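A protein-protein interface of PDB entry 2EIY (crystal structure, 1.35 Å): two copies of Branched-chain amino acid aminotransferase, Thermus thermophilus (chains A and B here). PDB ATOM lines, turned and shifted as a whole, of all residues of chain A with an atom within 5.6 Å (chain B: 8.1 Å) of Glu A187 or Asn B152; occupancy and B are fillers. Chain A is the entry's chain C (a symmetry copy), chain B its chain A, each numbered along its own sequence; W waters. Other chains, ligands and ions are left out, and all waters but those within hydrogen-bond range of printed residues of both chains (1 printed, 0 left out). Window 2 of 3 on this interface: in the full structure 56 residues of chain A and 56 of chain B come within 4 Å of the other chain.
Pro A150 touches Glu B187, and with the chains exchanged Glu A187 touches Pro B150.
Of the 11 pairs that touch across the chains among the printed residues, 2 have their exchanged pair printed and touching as well.
Glu A187 touches three residues of chain B.
Of chain A, only Ser A145 (3.98 Å), Trp A146 (3.3 Å), Ala A147 (2.9 Å) and Glu A187 (2.6 Å) come within 4 Å of Asn B152.
Of the printed residues of chain B, Pro A150 touches Glu B187.
Of the printed residues of chain B, Ser A145 touches Asn B152.
Gly B156 touches none of the printed residues of chain A.
Arg A148 touches none of the printed residues of chain B.
The nearest residue of chain B that does not touch Glu A187 is Ala B151 (5.5 Å).
The nearest residue of chain A that does not touch Asn B152 is Asn A166 (4.8 Å).
Among the printed residues, pairs that only touch across the chains: Ser A145 with Asn B152 (3.98 Å), Trp A146 with Asn B152 (3.3 Å), Trp A146 with Val B153 (3.8 Å), Ala A147 with Val B153 (3.6 Å), Pro A150 with Glu B187 (3.0 Å), Asn A166 with Met B154 (3.99 Å), Glu A187 with Pro B150 (3.1 Å) and Glu A187 with Val B153 (3.6 Å).
Of the 11 printed residues of chain A, 6 touch a printed residue of chain B.
Printed residues of chain B that touch a printed residue of chain A: Pro B150, Asn B152, Val B153, Met B154 and Glu B187.
Along chain B the printed residues that touch a printed residue of chain A span positions 150 to 187.
The side-chain amide nitrogen of Asn A166 sits at hydrogen-bond distance from the backbone carbonyl oxygen of Val B153 (2.8 Å).
The backbone NH (N) of Ala A147 is in hydrogen-bond range of the backbone carbonyl oxygen (O) of Asn B152.
The side-chain amide oxygen (OD1) of Asn B152 sits close to the side-chain carboxylate (OE2) of Glu A187.
The backbone carbonyl oxygen of Ala A147 is in hydrogen-bond range of the side-chain amide nitrogen of Asn A166, 2.9 Å away.
Water W1 lies within hydrogen-bond range of O of Ser A145 (2.7 Å) and ND2 of Asn B152 (2.9 Å).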
ATOM      1  N   SER A 145       0.978  -9.822 -18.065  1.00  0.00           N
ATOM      2  CA  SER A 145       1.560 -10.503 -19.214  1.00  0.00           C
ATOM      3  C   SER A 145       3.083 -10.538 -19.021  1.00  0.00           C
ATOM      4  O   SER A 145       3.812 -11.043 -19.874  1.00  0.00           O
ATOM      5  CB  SER A 145       1.202  -9.779 -20.510  1.00  0.00           C
ATOM      6  OG  SER A 145       1.779  -8.488 -20.535  1.00  0.00           O
ATOM      7  N   TRP A 146       3.555  -9.983 -17.905  1.00  0.00           N
ATOM      8  CA  TRP A 146       4.978 -10.010 -17.564  1.00  0.00           C
ATOM      9  C   TRP A 146       5.121 -11.020 -16.428  1.00  0.00           C
ATOM     10  O   TRP A 146       4.394 -10.954 -15.434  1.00  0.00           O
ATOM     11  CB  TRP A 146       5.475  -8.633 -17.100  1.00  0.00           C
ATOM     12  CG  TRP A 146       5.524  -7.623 -18.201  1.00  0.00           C
ATOM     13  CD1 TRP A 146       4.539  -6.747 -18.551  1.00  0.00           C
ATOM     14  CD2 TRP A 146       6.582  -7.437 -19.153  1.00  0.00           C
ATOM     15  NE1 TRP A 146       4.912  -6.032 -19.664  1.00  0.00           N
ATOM     16  CE2 TRP A 146       6.161  -6.435 -20.054  1.00  0.00           C
ATOM     17  CE3 TRP A 146       7.843  -8.025 -19.334  1.00  0.00           C
ATOM     18  CZ2 TRP A 146       6.955  -6.005 -21.123  1.00  0.00           C
ATOM     19  CZ3 TRP A 146       8.633  -7.597 -20.402  1.00  0.00           C
ATOM     20  CH2 TRP A 146       8.183  -6.598 -21.281  1.00  0.00           C
ATOM     21  N   ALA A 147       6.037 -11.968 -16.588  1.00  0.00           N
ATOM     22  CA  ALA A 147       6.258 -12.993 -15.574  1.00  0.00           C
ATOM     23  C   ALA A 147       7.343 -12.561 -14.604  1.00  0.00           C
ATOM     24  O   ALA A 147       8.297 -11.893 -15.004  1.00  0.00           O
ATOM     25  CB  ALA A 147       6.665 -14.312 -16.247  1.00  0.00           C
ATOM     26  N   ARG A 148       7.201 -12.912 -13.328  1.00  0.00           N
ATOM     27  CA  ARG A 148       8.250 -12.559 -12.381  1.00  0.00           C
ATOM     28  C   ARG A 148       9.457 -13.403 -12.775  1.00  0.00           C
ATOM     29  O   ARG A 148       9.331 -14.577 -13.127  1.00  0.00           O
ATOM     30  CB  ARG A 148       7.848 -12.838 -10.926  1.00  0.00           C
ATOM     31  CG  ARG A 148       8.942 -12.407  -9.937  1.00  0.00           C
ATOM     32  CD  ARG A 148       8.453 -12.239  -8.508  1.00  0.00           C
ATOM     33  NE  ARG A 148       9.556 -11.950  -7.586  1.00  0.00           N
ATOM     34  CZ  ARG A 148      10.030 -10.735  -7.311  1.00  0.00           C
ATOM     35  NH1 ARG A 148       9.508  -9.658  -7.881  1.00  0.00           N
ATOM     36  NH2 ARG A 148      11.026 -10.594  -6.442  1.00  0.00           N
ATOM     37  N   PRO A 150      12.772 -15.703 -13.235  1.00  0.00           N
ATOM     38  CA  PRO A 150      13.217 -16.988 -12.695  1.00  0.00           C
ATOM     39  C   PRO A 150      14.342 -16.699 -11.695  1.00  0.00           C
ATOM     40  O   PRO A 150      15.010 -15.656 -11.773  1.00  0.00           O
ATOM     41  CB  PRO A 150      13.723 -17.716 -13.931  1.00  0.00           C
ATOM     42  CG  PRO A 150      12.766 -17.267 -14.983  1.00  0.00           C
ATOM     43  CD  PRO A 150      12.652 -15.770 -14.704  1.00  0.00           C
ATOM     44  N   ASN A 166      10.683  -4.966 -13.873  1.00  0.00           N
ATOM     45  CA  ASN A 166       9.669  -6.006 -14.044  1.00  0.00           C
ATOM     46  C   ASN A 166       8.396  -5.581 -13.297  1.00  0.00           C
ATOM     47  O   ASN A 166       7.293  -5.654 -13.844  1.00  0.00           O
ATOM     48  CB  ASN A 166      10.235  -7.344 -13.523  1.00  0.00           C
ATOM     49  CG  ASN A 166       9.242  -8.495 -13.606  1.00  0.00           C
ATOM     50  OD1 ASN A 166       8.616  -8.861 -12.612  1.00  0.00           O
ATOM     51  ND2 ASN A 166       9.105  -9.078 -14.791  1.00  0.00           N
ATOM     52  N   LEU A 185       2.614 -14.019 -12.627  1.00  0.00           N
ATOM     53  CA  LEU A 185       2.786 -15.464 -12.591  1.00  0.00           C
ATOM     54  C   LEU A 185       4.277 -15.689 -12.807  1.00  0.00           C
ATOM     55  O   LEU A 185       4.988 -14.767 -13.224  1.00  0.00           O
ATOM     56  CB  LEU A 185       2.035 -16.134 -13.746  1.00  0.00           C
ATOM     57  CG  LEU A 185       0.544 -15.840 -13.916  1.00  0.00           C
ATOM     58  CD1 LEU A 185       0.012 -16.616 -15.120  1.00  0.00           C
ATOM     59  CD2 LEU A 185      -0.201 -16.233 -12.652  1.00  0.00           C
ATOM     60  N   ASP A 186       4.763 -16.889 -12.502  1.00  0.00           N
ATOM     61  CA  ASP A 186       6.162 -17.183 -12.784  1.00  0.00           C
ATOM     62  C   ASP A 186       6.191 -17.695 -14.229  1.00  0.00           C
ATOM     63  O   ASP A 186       5.140 -17.824 -14.863  1.00  0.00           O
ATOM     64  CB  ASP A 186       6.774 -18.205 -11.798  1.00  0.00           C
ATOM     65  CG  ASP A 186       5.993 -19.506 -11.696  1.00  0.00           C
ATOM     66  OD1 ASP A 186       5.368 -19.938 -12.685  1.00  0.00           O
ATOM     67  OD2 ASP A 186       6.040 -20.112 -10.600  1.00  0.00           O
ATOM     68  N   GLU A 187       7.373 -17.968 -14.768  1.00  0.00           N
ATOM     69  CA  GLU A 187       7.469 -18.408 -16.159  1.00  0.00           C
ATOM     70  C   GLU A 187       6.741 -19.724 -16.443  1.00  0.00           C
ATOM     71  O   GLU A 187       6.316 -19.970 -17.577  1.00  0.00           O
ATOM     72  CB  GLU A 187       8.942 -18.527 -16.569  1.00  0.00           C
ATOM     73  CG  GLU A 187       9.184 -18.545 -18.074  1.00  0.00           C
ATOM     74  CD  GLU A 187       8.670 -17.296 -18.772  1.00  0.00           C
ATOM     75  OE1 GLU A 187       7.471 -17.249 -19.121  1.00  0.00           O
ATOM     76  OE2 GLU A 187       9.466 -16.347 -18.961  1.00  0.00           O
ATOM     77  N   GLU A 188       6.591 -20.553 -15.416  1.00  0.00           N
ATOM     78  CA  GLU A 188       5.912 -21.839 -15.557  1.00  0.00           C
ATOM     79  C   GLU A 188       4.389 -21.710 -15.562  1.00  0.00           C
ATOM     80  O   GLU A 188       3.681 -22.669 -15.873  1.00  0.00           O
ATOM     81  CB  GLU A 188       6.337 -22.790 -14.436  1.00  0.00           C
ATOM     82  CG  GLU A 188       7.774 -23.292 -14.537  1.00  0.00           C
ATOM     83  CD  GLU A 188       8.801 -22.186 -14.382  1.00  0.00           C
ATOM     84  OE1 GLU A 188       8.680 -21.391 -13.428  1.00  0.00           O
ATOM     85  OE2 GLU A 188       9.735 -22.117 -15.208  1.00  0.00           O
ATOM     86  N   GLY A 189       3.885 -20.540 -15.181  1.00  0.00           N
ATOM     87  CA  GLY A 189       2.448 -20.326 -15.186  1.00  0.00           C
ATOM     88  C   GLY A 189       1.757 -20.288 -13.836  1.00  0.00           C
ATOM     89  O   GLY A 189       0.546 -20.078 -13.780  1.00  0.00           O
ATOM     90  N   PHE B 149      17.415 -13.016 -19.389  1.00  0.00           N
ATOM     91  CA  PHE B 149      15.980 -13.011 -19.140  1.00  0.00           C
ATOM     92  C   PHE B 149      15.060 -13.345 -20.306  1.00  0.00           C
ATOM     93  O   PHE B 149      15.311 -12.965 -21.451  1.00  0.00           O
ATOM     94  CB  PHE B 149      15.561 -11.651 -18.563  1.00  0.00           C
ATOM     95  CG  PHE B 149      16.442 -10.513 -18.996  1.00  0.00           C
ATOM     96  CD1 PHE B 149      16.493 -10.115 -20.325  1.00  0.00           C
ATOM     97  CD2 PHE B 149      17.261  -9.869 -18.072  1.00  0.00           C
ATOM     98  CE1 PHE B 149      17.351  -9.095 -20.732  1.00  0.00           C
ATOM     99  CE2 PHE B 149      18.120  -8.850 -18.472  1.00  0.00           C
ATOM    100  CZ  PHE B 149      18.164  -8.465 -19.801  1.00  0.00           C
ATOM    101  N   PRO B 150      13.989 -14.103 -20.024  1.00  0.00           N
ATOM    102  CA  PRO B 150      13.020 -14.464 -21.059  1.00  0.00           C
ATOM    103  C   PRO B 150      12.409 -13.163 -21.591  1.00  0.00           C
ATOM    104  O   PRO B 150      12.420 -12.133 -20.903  1.00  0.00           O
ATOM    105  CB  PRO B 150      12.004 -15.299 -20.295  1.00  0.00           C
ATOM    106  CG  PRO B 150      12.856 -16.024 -19.311  1.00  0.00           C
ATOM    107  CD  PRO B 150      13.795 -14.930 -18.817  1.00  0.00           C
ATOM    108  N   ALA B 151      11.863 -13.221 -22.802  1.00  0.00           N
ATOM    109  CA  ALA B 151      11.288 -12.059 -23.467  1.00  0.00           C
ATOM    110  C   ALA B 151      10.046 -11.466 -22.820  1.00  0.00           C
ATOM    111  O   ALA B 151       9.581 -10.397 -23.236  1.00  0.00           O
ATOM    112  CB  ALA B 151      11.003 -12.397 -24.922  1.00  0.00           C
ATOM    113  N   ASN B 152       9.500 -12.160 -21.827  1.00  0.00           N
ATOM    114  CA  ASN B 152       8.324 -11.675 -21.110  1.00  0.00           C
ATOM    115  C   ASN B 152       8.662 -11.413 -19.642  1.00  0.00           C
ATOM    116  O   ASN B 152       7.768 -11.342 -18.797  1.00  0.00           O
ATOM    117  CB  ASN B 152       7.178 -12.689 -21.210  1.00  0.00           C
ATOM    118  CG  ASN B 152       7.500 -14.004 -20.530  1.00  0.00           C
ATOM    119  OD1 ASN B 152       8.668 -14.356 -20.359  1.00  0.00           O
ATOM    120  ND2 ASN B 152       6.464 -14.745 -20.148  1.00  0.00           N
ATOM    121  N   VAL B 153       9.955 -11.276 -19.347  1.00  0.00           N
ATOM    122  CA  VAL B 153      10.423 -11.008 -17.988  1.00  0.00           C
ATOM    123  C   VAL B 153      11.086  -9.626 -17.931  1.00  0.00           C
ATOM    124  O   VAL B 153      10.794  -8.822 -17.044  1.00  0.00           O
ATOM    125  CB  VAL B 153      11.400 -12.111 -17.527  1.00  0.00           C
ATOM    126  CG1 VAL B 153      12.096 -11.705 -16.231  1.00  0.00           C
ATOM    127  CG2 VAL B 153      10.625 -13.412 -17.319  1.00  0.00           C
ATOM    128  N   MET B 154      11.987  -9.362 -18.873  1.00  0.00           N
ATOM    129  CA  MET B 154      12.645  -8.059 -18.982  1.00  0.00           C
ATOM    130  C   MET B 154      12.700  -7.800 -20.488  1.00  0.00           C
ATOM    131  O   MET B 154      12.797  -8.741 -21.274  1.00  0.00           O
ATOM    132  CB  MET B 154      14.059  -8.087 -18.382  1.00  0.00           C
ATOM    133  CG  MET B 154      14.120  -8.332 -16.864  1.00  0.00           C
ATOM    134  SD  MET B 154      13.548  -6.963 -15.809  1.00  0.00           S
ATOM    135  CE  MET B 154      15.059  -5.996 -15.655  1.00  0.00           C
ATOM    136  N   PRO B 155      12.613  -6.528 -20.910  1.00  0.00           N
ATOM    137  CA  PRO B 155      12.648  -6.149 -22.329  1.00  0.00           C
ATOM    138  C   PRO B 155      14.059  -6.222 -22.900  1.00  0.00           C
ATOM    139  O   PRO B 155      14.782  -5.225 -22.919  1.00  0.00           O
ATOM    140  CB  PRO B 155      12.095  -4.729 -22.312  1.00  0.00           C
ATOM    141  CG  PRO B 155      12.621  -4.197 -21.016  1.00  0.00           C
ATOM    142  CD  PRO B 155      12.402  -5.346 -20.054  1.00  0.00           C
ATOM    143  N   GLY B 156      14.424  -7.409 -23.379  1.00  0.00           N
ATOM    144  CA  GLY B 156      15.757  -7.648 -23.907  1.00  0.00           C
ATOM    145  C   GLY B 156      16.161  -6.972 -25.201  1.00  0.00           C
ATOM    146  O   GLY B 156      17.320  -7.076 -25.605  1.00  0.00           O
ATOM    147  N   GLU B 187      16.955 -19.330 -20.740  1.00  0.00           N
ATOM    148  CA  GLU B 187      16.413 -20.270 -19.765  1.00  0.00           C
ATOM    149  C   GLU B 187      16.240 -21.688 -20.303  1.00  0.00           C
ATOM    150  O   GLU B 187      16.248 -22.652 -19.534  1.00  0.00           O
ATOM    151  CB  GLU B 187      15.078 -19.743 -19.224  1.00  0.00           C
ATOM    152  CG  GLU B 187      14.627 -20.361 -17.898  1.00  0.00           C
ATOM    153  CD  GLU B 187      15.613 -20.117 -16.764  1.00  0.00           C
ATOM    154  OE1 GLU B 187      16.580 -20.892 -16.631  1.00  0.00           O
ATOM    155  OE2 GLU B 187      15.431 -19.137 -16.004  1.00  0.00           O
ATOM    156  N   GLU B 188      16.097 -21.815 -21.619  1.00  0.00           N
ATOM    157  CA  GLU B 188      15.928 -23.122 -22.240  1.00  0.00           C
ATOM    158  C   GLU B 188      17.256 -23.853 -22.423  1.00  0.00           C
ATOM    159  O   GLU B 188      17.274 -25.041 -22.744  1.00  0.00           O
ATOM    160  CB  GLU B 188      15.218 -22.981 -23.589  1.00  0.00           C
ATOM    161  CG  GLU B 188      13.741 -22.590 -23.499  1.00  0.00           C
ATOM    162  CD  GLU B 188      13.515 -21.222 -22.875  1.00  0.00           C
ATOM    163  OE1 GLU B 188      14.220 -20.264 -23.251  1.00  0.00           O
ATOM    164  OE2 GLU B 188      12.619 -21.100 -22.014  1.00  0.00           O
ATOM    165  N   VAL B 214      16.435 -13.625 -27.216  1.00  0.00           N
ATOM    166  CA  VAL B 214      16.208 -12.664 -26.131  1.00  0.00           C
ATOM    167  C   VAL B 214      17.325 -11.622 -26.040  1.00  0.00           C
ATOM    168  O   VAL B 214      17.409 -10.875 -25.062  1.00  0.00           O
ATOM    169  CB  VAL B 214      16.113 -13.373 -24.755  1.00  0.00           C
ATOM    170  CG1 VAL B 214      14.839 -14.203 -24.680  1.00  0.00           C
ATOM    171  CG2 VAL B 214      17.343 -14.254 -24.532  1.00  0.00           C
HETATM  172  O   HOH W   1       3.742 -13.764 -19.985  1.00  0.00           O
